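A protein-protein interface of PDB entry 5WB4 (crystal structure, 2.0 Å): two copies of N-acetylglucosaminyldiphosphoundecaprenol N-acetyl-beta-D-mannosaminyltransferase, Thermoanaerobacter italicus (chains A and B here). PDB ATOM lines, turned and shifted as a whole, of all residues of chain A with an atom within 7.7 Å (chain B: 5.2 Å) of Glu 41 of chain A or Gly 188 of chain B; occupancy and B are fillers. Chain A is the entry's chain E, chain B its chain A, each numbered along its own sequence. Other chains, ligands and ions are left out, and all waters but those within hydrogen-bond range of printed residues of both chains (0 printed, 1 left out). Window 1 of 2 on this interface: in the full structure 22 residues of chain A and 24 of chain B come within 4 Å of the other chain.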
ATOM      1  N   PRO A  38     -24.050  11.509  16.214  1.00  0.00           N
ATOM      2  CA  PRO A  38     -24.566  12.693  16.908  1.00  0.00           C
ATOM      3  C   PRO A  38     -23.976  12.903  18.291  1.00  0.00           C
ATOM      4  O   PRO A  38     -23.787  11.956  19.061  1.00  0.00           O
ATOM      5  CB  PRO A  38     -26.088  12.461  16.946  1.00  0.00           C
ATOM      6  CG  PRO A  38     -26.353  11.393  15.918  1.00  0.00           C
ATOM      7  CD  PRO A  38     -25.139  10.531  15.965  1.00  0.00           C
ATOM      8  N   ASN A  39     -23.657  14.169  18.571  1.00  0.00           N
ATOM      9  CA  ASN A  39     -23.151  14.648  19.851  1.00  0.00           C
ATOM     10  C   ASN A  39     -24.117  15.731  20.354  1.00  0.00           C
ATOM     11  O   ASN A  39     -25.093  16.053  19.663  1.00  0.00           O
ATOM     12  CB  ASN A  39     -21.710  15.194  19.696  1.00  0.00           C
ATOM     13  CG  ASN A  39     -21.511  16.151  18.554  1.00  0.00           C
ATOM     14  OD1 ASN A  39     -22.368  16.993  18.238  1.00  0.00           O
ATOM     15  ND2 ASN A  39     -20.373  16.023  17.886  1.00  0.00           N
ATOM     16  N   ALA A  40     -23.828  16.322  21.535  1.00  0.00           N
ATOM     17  CA  ALA A  40     -24.657  17.379  22.134  1.00  0.00           C
ATOM     18  C   ALA A  40     -24.898  18.557  21.164  1.00  0.00           C
ATOM     19  O   ALA A  40     -26.031  19.022  21.032  1.00  0.00           O
ATOM     20  CB  ALA A  40     -23.998  17.882  23.427  1.00  0.00           C
ATOM     21  N   GLU A  41     -23.830  19.000  20.461  1.00  0.00           N
ATOM     22  CA  GLU A  41     -23.869  20.113  19.507  1.00  0.00           C
ATOM     23  C   GLU A  41     -24.831  19.815  18.348  1.00  0.00           C
ATOM     24  O   GLU A  41     -25.633  20.666  17.981  1.00  0.00           O
ATOM     25  CB  GLU A  41     -22.433  20.414  19.020  1.00  0.00           C
ATOM     26  CG  GLU A  41     -22.343  21.412  17.878  1.00  0.00           C
ATOM     27  CD  GLU A  41     -22.371  22.874  18.282  1.00  0.00           C
ATOM     28  OE1 GLU A  41     -21.433  23.318  18.985  1.00  0.00           O
ATOM     29  OE2 GLU A  41     -23.296  23.589  17.833  1.00  0.00           O
ATOM     30  N   ILE A  42     -24.755  18.603  17.789  1.00  0.00           N
ATOM     31  CA  ILE A  42     -25.632  18.151  16.697  1.00  0.00           C
ATOM     32  C   ILE A  42     -27.099  18.129  17.154  1.00  0.00           C
ATOM     33  O   ILE A  42     -27.968  18.611  16.415  1.00  0.00           O
ATOM     34  CB  ILE A  42     -25.124  16.793  16.134  1.00  0.00           C
ATOM     35  CG1 ILE A  42     -23.890  17.058  15.236  1.00  0.00           C
ATOM     36  CG2 ILE A  42     -26.260  15.986  15.401  1.00  0.00           C
ATOM     37  CD1 ILE A  42     -23.052  15.805  14.839  1.00  0.00           C
ATOM     38  N   VAL A  43     -27.358  17.605  18.389  1.00  0.00           N
ATOM     39  CA  VAL A  43     -28.702  17.579  18.979  1.00  0.00           C
ATOM     40  C   VAL A  43     -29.280  19.001  19.014  1.00  0.00           C
ATOM     41  O   VAL A  43     -30.410  19.207  18.573  1.00  0.00           O
ATOM     42  CB  VAL A  43     -28.743  16.852  20.352  1.00  0.00           C
ATOM     43  CG1 VAL A  43     -30.034  17.138  21.125  1.00  0.00           C
ATOM     44  CG2 VAL A  43     -28.569  15.356  20.168  1.00  0.00           C
ATOM     45  N   MET A  44     -28.475  19.981  19.497  1.00  0.00           N
ATOM     46  CA  MET A  44     -28.866  21.384  19.554  1.00  0.00           C
ATOM     47  C   MET A  44     -29.186  21.934  18.149  1.00  0.00           C
ATOM     48  O   MET A  44     -30.228  22.583  17.985  1.00  0.00           O
ATOM     49  CB  MET A  44     -27.787  22.227  20.239  1.00  0.00           C
ATOM     50  CG  MET A  44     -28.123  23.698  20.277  1.00  0.00           C
ATOM     51  SD  MET A  44     -26.840  24.705  21.300  1.00  0.00           S
ATOM     52  CE  MET A  44     -25.531  24.943  19.981  1.00  0.00           C
ATOM     53  N   MET A  45     -28.306  21.686  17.149  1.00  0.00           N
ATOM     54  CA  MET A  45     -28.502  22.146  15.764  1.00  0.00           C
ATOM     55  C   MET A  45     -29.829  21.657  15.184  1.00  0.00           C
ATOM     56  O   MET A  45     -30.568  22.456  14.624  1.00  0.00           O
ATOM     57  CB  MET A  45     -27.366  21.662  14.849  1.00  0.00           C
ATOM     58  CG  MET A  45     -26.034  22.323  15.103  1.00  0.00           C
ATOM     59  SD  MET A  45     -24.635  21.355  14.128  1.00  0.00           S
ATOM     60  CE  MET A  45     -23.705  22.966  13.577  1.00  0.00           C
ATOM     61  N   ALA A  46     -30.128  20.343  15.347  1.00  0.00           N
ATOM     62  CA  ALA A  46     -31.341  19.654  14.872  1.00  0.00           C
ATOM     63  C   ALA A  46     -32.643  20.226  15.441  1.00  0.00           C
ATOM     64  O   ALA A  46     -33.686  20.083  14.813  1.00  0.00           O
ATOM     65  CB  ALA A  46     -31.247  18.171  15.164  1.00  0.00           C
ATOM     66  N   GLN A  47     -32.591  20.885  16.614  1.00  0.00           N
ATOM     67  CA  GLN A  47     -33.784  21.532  17.200  1.00  0.00           C
ATOM     68  C   GLN A  47     -34.231  22.731  16.339  1.00  0.00           C
ATOM     69  O   GLN A  47     -35.408  23.080  16.335  1.00  0.00           O
ATOM     70  CB  GLN A  47     -33.502  22.017  18.639  1.00  0.00           C
ATOM     71  CG  GLN A  47     -32.959  20.959  19.604  1.00  0.00           C
ATOM     72  CD  GLN A  47     -33.757  19.671  19.628  1.00  0.00           C
ATOM     73  OE1 GLN A  47     -34.975  19.664  19.848  1.00  0.00           O
ATOM     74  NE2 GLN A  47     -33.080  18.543  19.400  1.00  0.00           N
ATOM     75  N   TYR A  52     -32.195  18.938   8.795  1.00  0.00           N
ATOM     76  CA  TYR A  52     -31.154  18.180   9.487  1.00  0.00           C
ATOM     77  C   TYR A  52     -31.775  17.118  10.378  1.00  0.00           C
ATOM     78  O   TYR A  52     -31.332  15.961  10.348  1.00  0.00           O
ATOM     79  CB  TYR A  52     -30.258  19.128  10.310  1.00  0.00           C
ATOM     80  CG  TYR A  52     -28.968  18.515  10.817  1.00  0.00           C
ATOM     81  CD1 TYR A  52     -28.307  17.524  10.090  1.00  0.00           C
ATOM     82  CD2 TYR A  52     -28.375  18.969  11.991  1.00  0.00           C
ATOM     83  CE1 TYR A  52     -27.130  16.941  10.567  1.00  0.00           C
ATOM     84  CE2 TYR A  52     -27.193  18.400  12.471  1.00  0.00           C
ATOM     85  CZ  TYR A  52     -26.554  17.416  11.737  1.00  0.00           C
ATOM     86  OH  TYR A  52     -25.379  16.886  12.206  1.00  0.00           O
ATOM     87  N   ASP A  65     -21.720  10.309  20.120  1.00  0.00           N
ATOM     88  CA  ASP A  65     -20.387  10.921  20.141  1.00  0.00           C
ATOM     89  C   ASP A  65     -20.264  11.862  21.333  1.00  0.00           C
ATOM     90  O   ASP A  65     -21.140  12.691  21.541  1.00  0.00           O
ATOM     91  CB  ASP A  65     -20.062  11.649  18.814  1.00  0.00           C
ATOM     92  CG  ASP A  65     -18.753  12.433  18.849  1.00  0.00           C
ATOM     93  OD1 ASP A  65     -17.688  11.806  19.036  1.00  0.00           O
ATOM     94  OD2 ASP A  65     -18.801  13.672  18.788  1.00  0.00           O
ATOM     95  N   GLY A  68     -21.645  14.569  26.561  1.00  0.00           N
ATOM     96  CA  GLY A  68     -22.933  15.237  26.720  1.00  0.00           C
ATOM     97  C   GLY A  68     -24.127  14.380  26.357  1.00  0.00           C
ATOM     98  O   GLY A  68     -25.069  14.258  27.148  1.00  0.00           O
ATOM     99  N   ILE A  69     -24.078  13.742  25.171  1.00  0.00           N
ATOM    100  CA  ILE A  69     -25.180  12.888  24.699  1.00  0.00           C
ATOM    101  C   ILE A  69     -25.400  11.659  25.607  1.00  0.00           C
ATOM    102  O   ILE A  69     -26.553  11.265  25.820  1.00  0.00           O
ATOM    103  CB  ILE A  69     -25.050  12.523  23.199  1.00  0.00           C
ATOM    104  CG1 ILE A  69     -26.442  12.145  22.600  1.00  0.00           C
ATOM    105  CG2 ILE A  69     -23.969  11.470  22.924  1.00  0.00           C
ATOM    106  CD1 ILE A  69     -26.624  12.556  21.175  1.00  0.00           C
ATOM    107  N   ALA A 164     -20.427  18.972  10.607  1.00  0.00           N
ATOM    108  CA  ALA A 164     -21.880  18.882  10.769  1.00  0.00           C
ATOM    109  C   ALA A 164     -22.498  20.288  10.732  1.00  0.00           C
ATOM    110  O   ALA A 164     -21.898  21.204  11.299  1.00  0.00           O
ATOM    111  CB  ALA A 164     -22.216  18.184  12.078  1.00  0.00           C
ATOM    112  N   LEU B 162     -23.571  28.703  22.546  1.00  0.00           N
ATOM    113  CA  LEU B 162     -23.945  29.191  21.206  1.00  0.00           C
ATOM    114  C   LEU B 162     -23.390  28.339  20.066  1.00  0.00           C
ATOM    115  O   LEU B 162     -23.796  28.512  18.927  1.00  0.00           O
ATOM    116  CB  LEU B 162     -23.500  30.661  21.020  1.00  0.00           C
ATOM    117  CG  LEU B 162     -24.066  31.745  21.963  1.00  0.00           C
ATOM    118  CD1 LEU B 162     -23.521  33.119  21.591  1.00  0.00           C
ATOM    119  CD2 LEU B 162     -25.571  31.791  21.917  1.00  0.00           C
ATOM    120  N   GLY B 163     -22.425  27.466  20.373  1.00  0.00           N
ATOM    121  CA  GLY B 163     -21.782  26.623  19.374  1.00  0.00           C
ATOM    122  C   GLY B 163     -20.584  27.302  18.744  1.00  0.00           C
ATOM    123  O   GLY B 163     -20.538  28.531  18.646  1.00  0.00           O
ATOM    124  N   ALA B 164     -19.591  26.503  18.328  1.00  0.00           N
ATOM    125  CA  ALA B 164     -18.368  27.042  17.736  1.00  0.00           C
ATOM    126  C   ALA B 164     -18.574  27.335  16.244  1.00  0.00           C
ATOM    127  O   ALA B 164     -19.262  26.557  15.579  1.00  0.00           O
ATOM    128  CB  ALA B 164     -17.213  26.057  17.949  1.00  0.00           C
ATOM    129  N   VAL B 186     -19.690  26.553  25.503  1.00  0.00           N
ATOM    130  CA  VAL B 186     -20.030  25.172  25.908  1.00  0.00           C
ATOM    131  C   VAL B 186     -20.911  24.406  24.883  1.00  0.00           C
ATOM    132  O   VAL B 186     -21.385  23.317  25.189  1.00  0.00           O
ATOM    133  CB  VAL B 186     -20.648  25.112  27.339  1.00  0.00           C
ATOM    134  CG1 VAL B 186     -19.691  25.669  28.401  1.00  0.00           C
ATOM    135  CG2 VAL B 186     -22.001  25.831  27.393  1.00  0.00           C
ATOM    136  N   GLY B 187     -21.102  24.962  23.690  1.00  0.00           N
ATOM    137  CA  GLY B 187     -21.859  24.325  22.614  1.00  0.00           C
ATOM    138  C   GLY B 187     -23.240  23.808  22.983  1.00  0.00           C
ATOM    139  O   GLY B 187     -24.083  24.577  23.457  1.00  0.00           O
ATOM    140  N   GLY B 188     -23.444  22.491  22.791  1.00  0.00           N
ATOM    141  CA  GLY B 188     -24.722  21.836  23.065  1.00  0.00           C
ATOM    142  C   GLY B 188     -24.933  21.382  24.495  1.00  0.00           C
ATOM    143  O   GLY B 188     -25.922  20.703  24.769  1.00  0.00           O
ATOM    144  N   SER B 189     -24.022  21.771  25.425  1.00  0.00           N
ATOM    145  CA  SER B 189     -24.037  21.352  26.844  1.00  0.00           C
ATOM    146  C   SER B 189     -25.323  21.637  27.612  1.00  0.00           C
ATOM    147  O   SER B 189     -25.654  20.831  28.473  1.00  0.00           O
ATOM    148  CB  SER B 189     -22.857  21.939  27.604  1.00  0.00           C
ATOM    149  OG  SER B 189     -21.647  21.431  27.077  1.00  0.00           O
ATOM    150  N   PHE B 190     -26.039  22.758  27.340  1.00  0.00           N
ATOM    151  CA  PHE B 190     -27.291  23.049  28.061  1.00  0.00           C
ATOM    152  C   PHE B 190     -28.395  22.100  27.633  1.00  0.00           C
ATOM    153  O   PHE B 190     -29.144  21.630  28.493  1.00  0.00           O
ATOM    154  CB  PHE B 190     -27.775  24.505  27.851  1.00  0.00           C
ATOM    155  CG  PHE B 190     -26.921  25.656  28.356  1.00  0.00           C
ATOM    156  CD1 PHE B 190     -25.751  25.422  29.072  1.00  0.00           C
ATOM    157  CD2 PHE B 190     -27.302  26.973  28.129  1.00  0.00           C
ATOM    158  CE1 PHE B 190     -24.960  26.489  29.517  1.00  0.00           C
ATOM    159  CE2 PHE B 190     -26.515  28.037  28.575  1.00  0.00           C
ATOM    160  CZ  PHE B 190     -25.335  27.789  29.246  1.00  0.00           C
ATOM    161  N   ASP B 191     -28.492  21.805  26.307  1.00  0.00           N
ATOM    162  CA  ASP B 191     -29.522  20.924  25.745  1.00  0.00           C
ATOM    163  C   ASP B 191     -29.527  19.548  26.388  1.00  0.00           C
ATOM    164  O   ASP B 191     -30.584  19.064  26.788  1.00  0.00           O
ATOM    165  CB  ASP B 191     -29.356  20.803  24.221  1.00  0.00           C
ATOM    166  CG  ASP B 191     -29.675  22.081  23.485  1.00  0.00           C
ATOM    167  OD1 ASP B 191     -28.819  22.970  23.462  1.00  0.00           O
ATOM    168  OD2 ASP B 191     -30.791  22.192  22.959  1.00  0.00           O
ATOM    169  N   VAL B 192     -28.339  18.951  26.547  1.00  0.00           N
ATOM    170  CA  VAL B 192     -28.171  17.612  27.127  1.00  0.00           C
ATOM    171  C   VAL B 192     -28.335  17.581  28.665  1.00  0.00           C
ATOM    172  O   VAL B 192     -28.533  16.500  29.218  1.00  0.00           O
ATOM    173  CB  VAL B 192     -26.856  16.952  26.664  1.00  0.00           C
ATOM    174  CG1 VAL B 192     -26.937  16.588  25.185  1.00  0.00           C
ATOM    175  CG2 VAL B 192     -25.631  17.827  26.959  1.00  0.00           C
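The side-chain sulfur of Met 44 of chain A lies close to the side-chain carboxylate of Asp 191 of chain B, at 3.4 Å. The side-chain sulfur (SD) of Met 44 of chain A lies close to the backbone carbonyl oxygen (O) of Gly 187 of chain B, 3.5 Å away.
The backbone NH (N) of Glu 41 of chain A sits close to the side-chain amide oxygen (OD1) of Asn 39 of chain A (3.3 Å).
Among the printed residues, merely in contact across the chains: Gly 68 of chain A with Val 192 of chain B (3.3 Å), Glu 41 of chain A with Gly 163 of chain B (3.3 Å), Ala 40 of chain A with Val 192 of chain B (3.7 Å), Ala 40 of chain A with Gly 188 of chain B (3.7 Å), Glu 41 of chain A with Ala 164 of chain B (3.7 Å), Glu 41 of chain A with Gly 187 of chain B (3.8 Å), Glu 41 of chain A with Gly 188 of chain B (3.95 Å) and Met 44 of chain A with Gly 188 of chain B (3.98 Å).
Printed residues of chain B within 4 Å of Ala 40 of chain A: Gly 188 and Val 192. Glu 41 of chain A touches just these residues of chain B: Gly 163, Ala 164, Gly 187 and Gly 188. Of the printed residues of chain B, Gly 68 of chain A touches Val 192. Of the printed residues of chain A, Gly 163 of chain B touches Glu 41 (3.3 Å). Of chain A, only Glu 41 and Met 44 come within 4 Å of Gly 187 of chain B. Of chain A, only Ala 40 (3.7 Å), Glu 41 (3.95 Å) and Met 44 (3.98 Å) come within 4 Å of Gly 188 of chain B. Printed residues of chain A within 4 Å of Asp 191 of chain B: Met 44. Of the printed residues of chain A, Val 192 of chain B touches Ala 40 (3.7 Å) and Gly 68 (3.3 Å). The nearest residue of chain A that does not touch Gly 188 of chain B is Ile 42 of chain A (6.2 Å). The nearest printed residue of chain B that does not touch Met 44 of chain A is Leu 162 of chain B (4.02 Å).
Printed residues of chain B that touch a printed residue of chain A: Gly 163, Ala 164, Gly 187, Gly 188, Asp 191 and Val 192. Hydrophobic or aromatic side chains of chain B that line the printed part of chain A: Val 192. Along chain B the printed residues that touch a printed residue of chain A span positions 163 to 192. Hydrophobic or aromatic side chains of chain A that line the printed part of chain B: Ala 40 and Met 44. Among the printed residues, 10 pairs touch across the chains.
1 position is printed for both chains. Of the 10 pairs that touch across the chains among the printed residues, none has its exchanged pair printed and touching as well.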
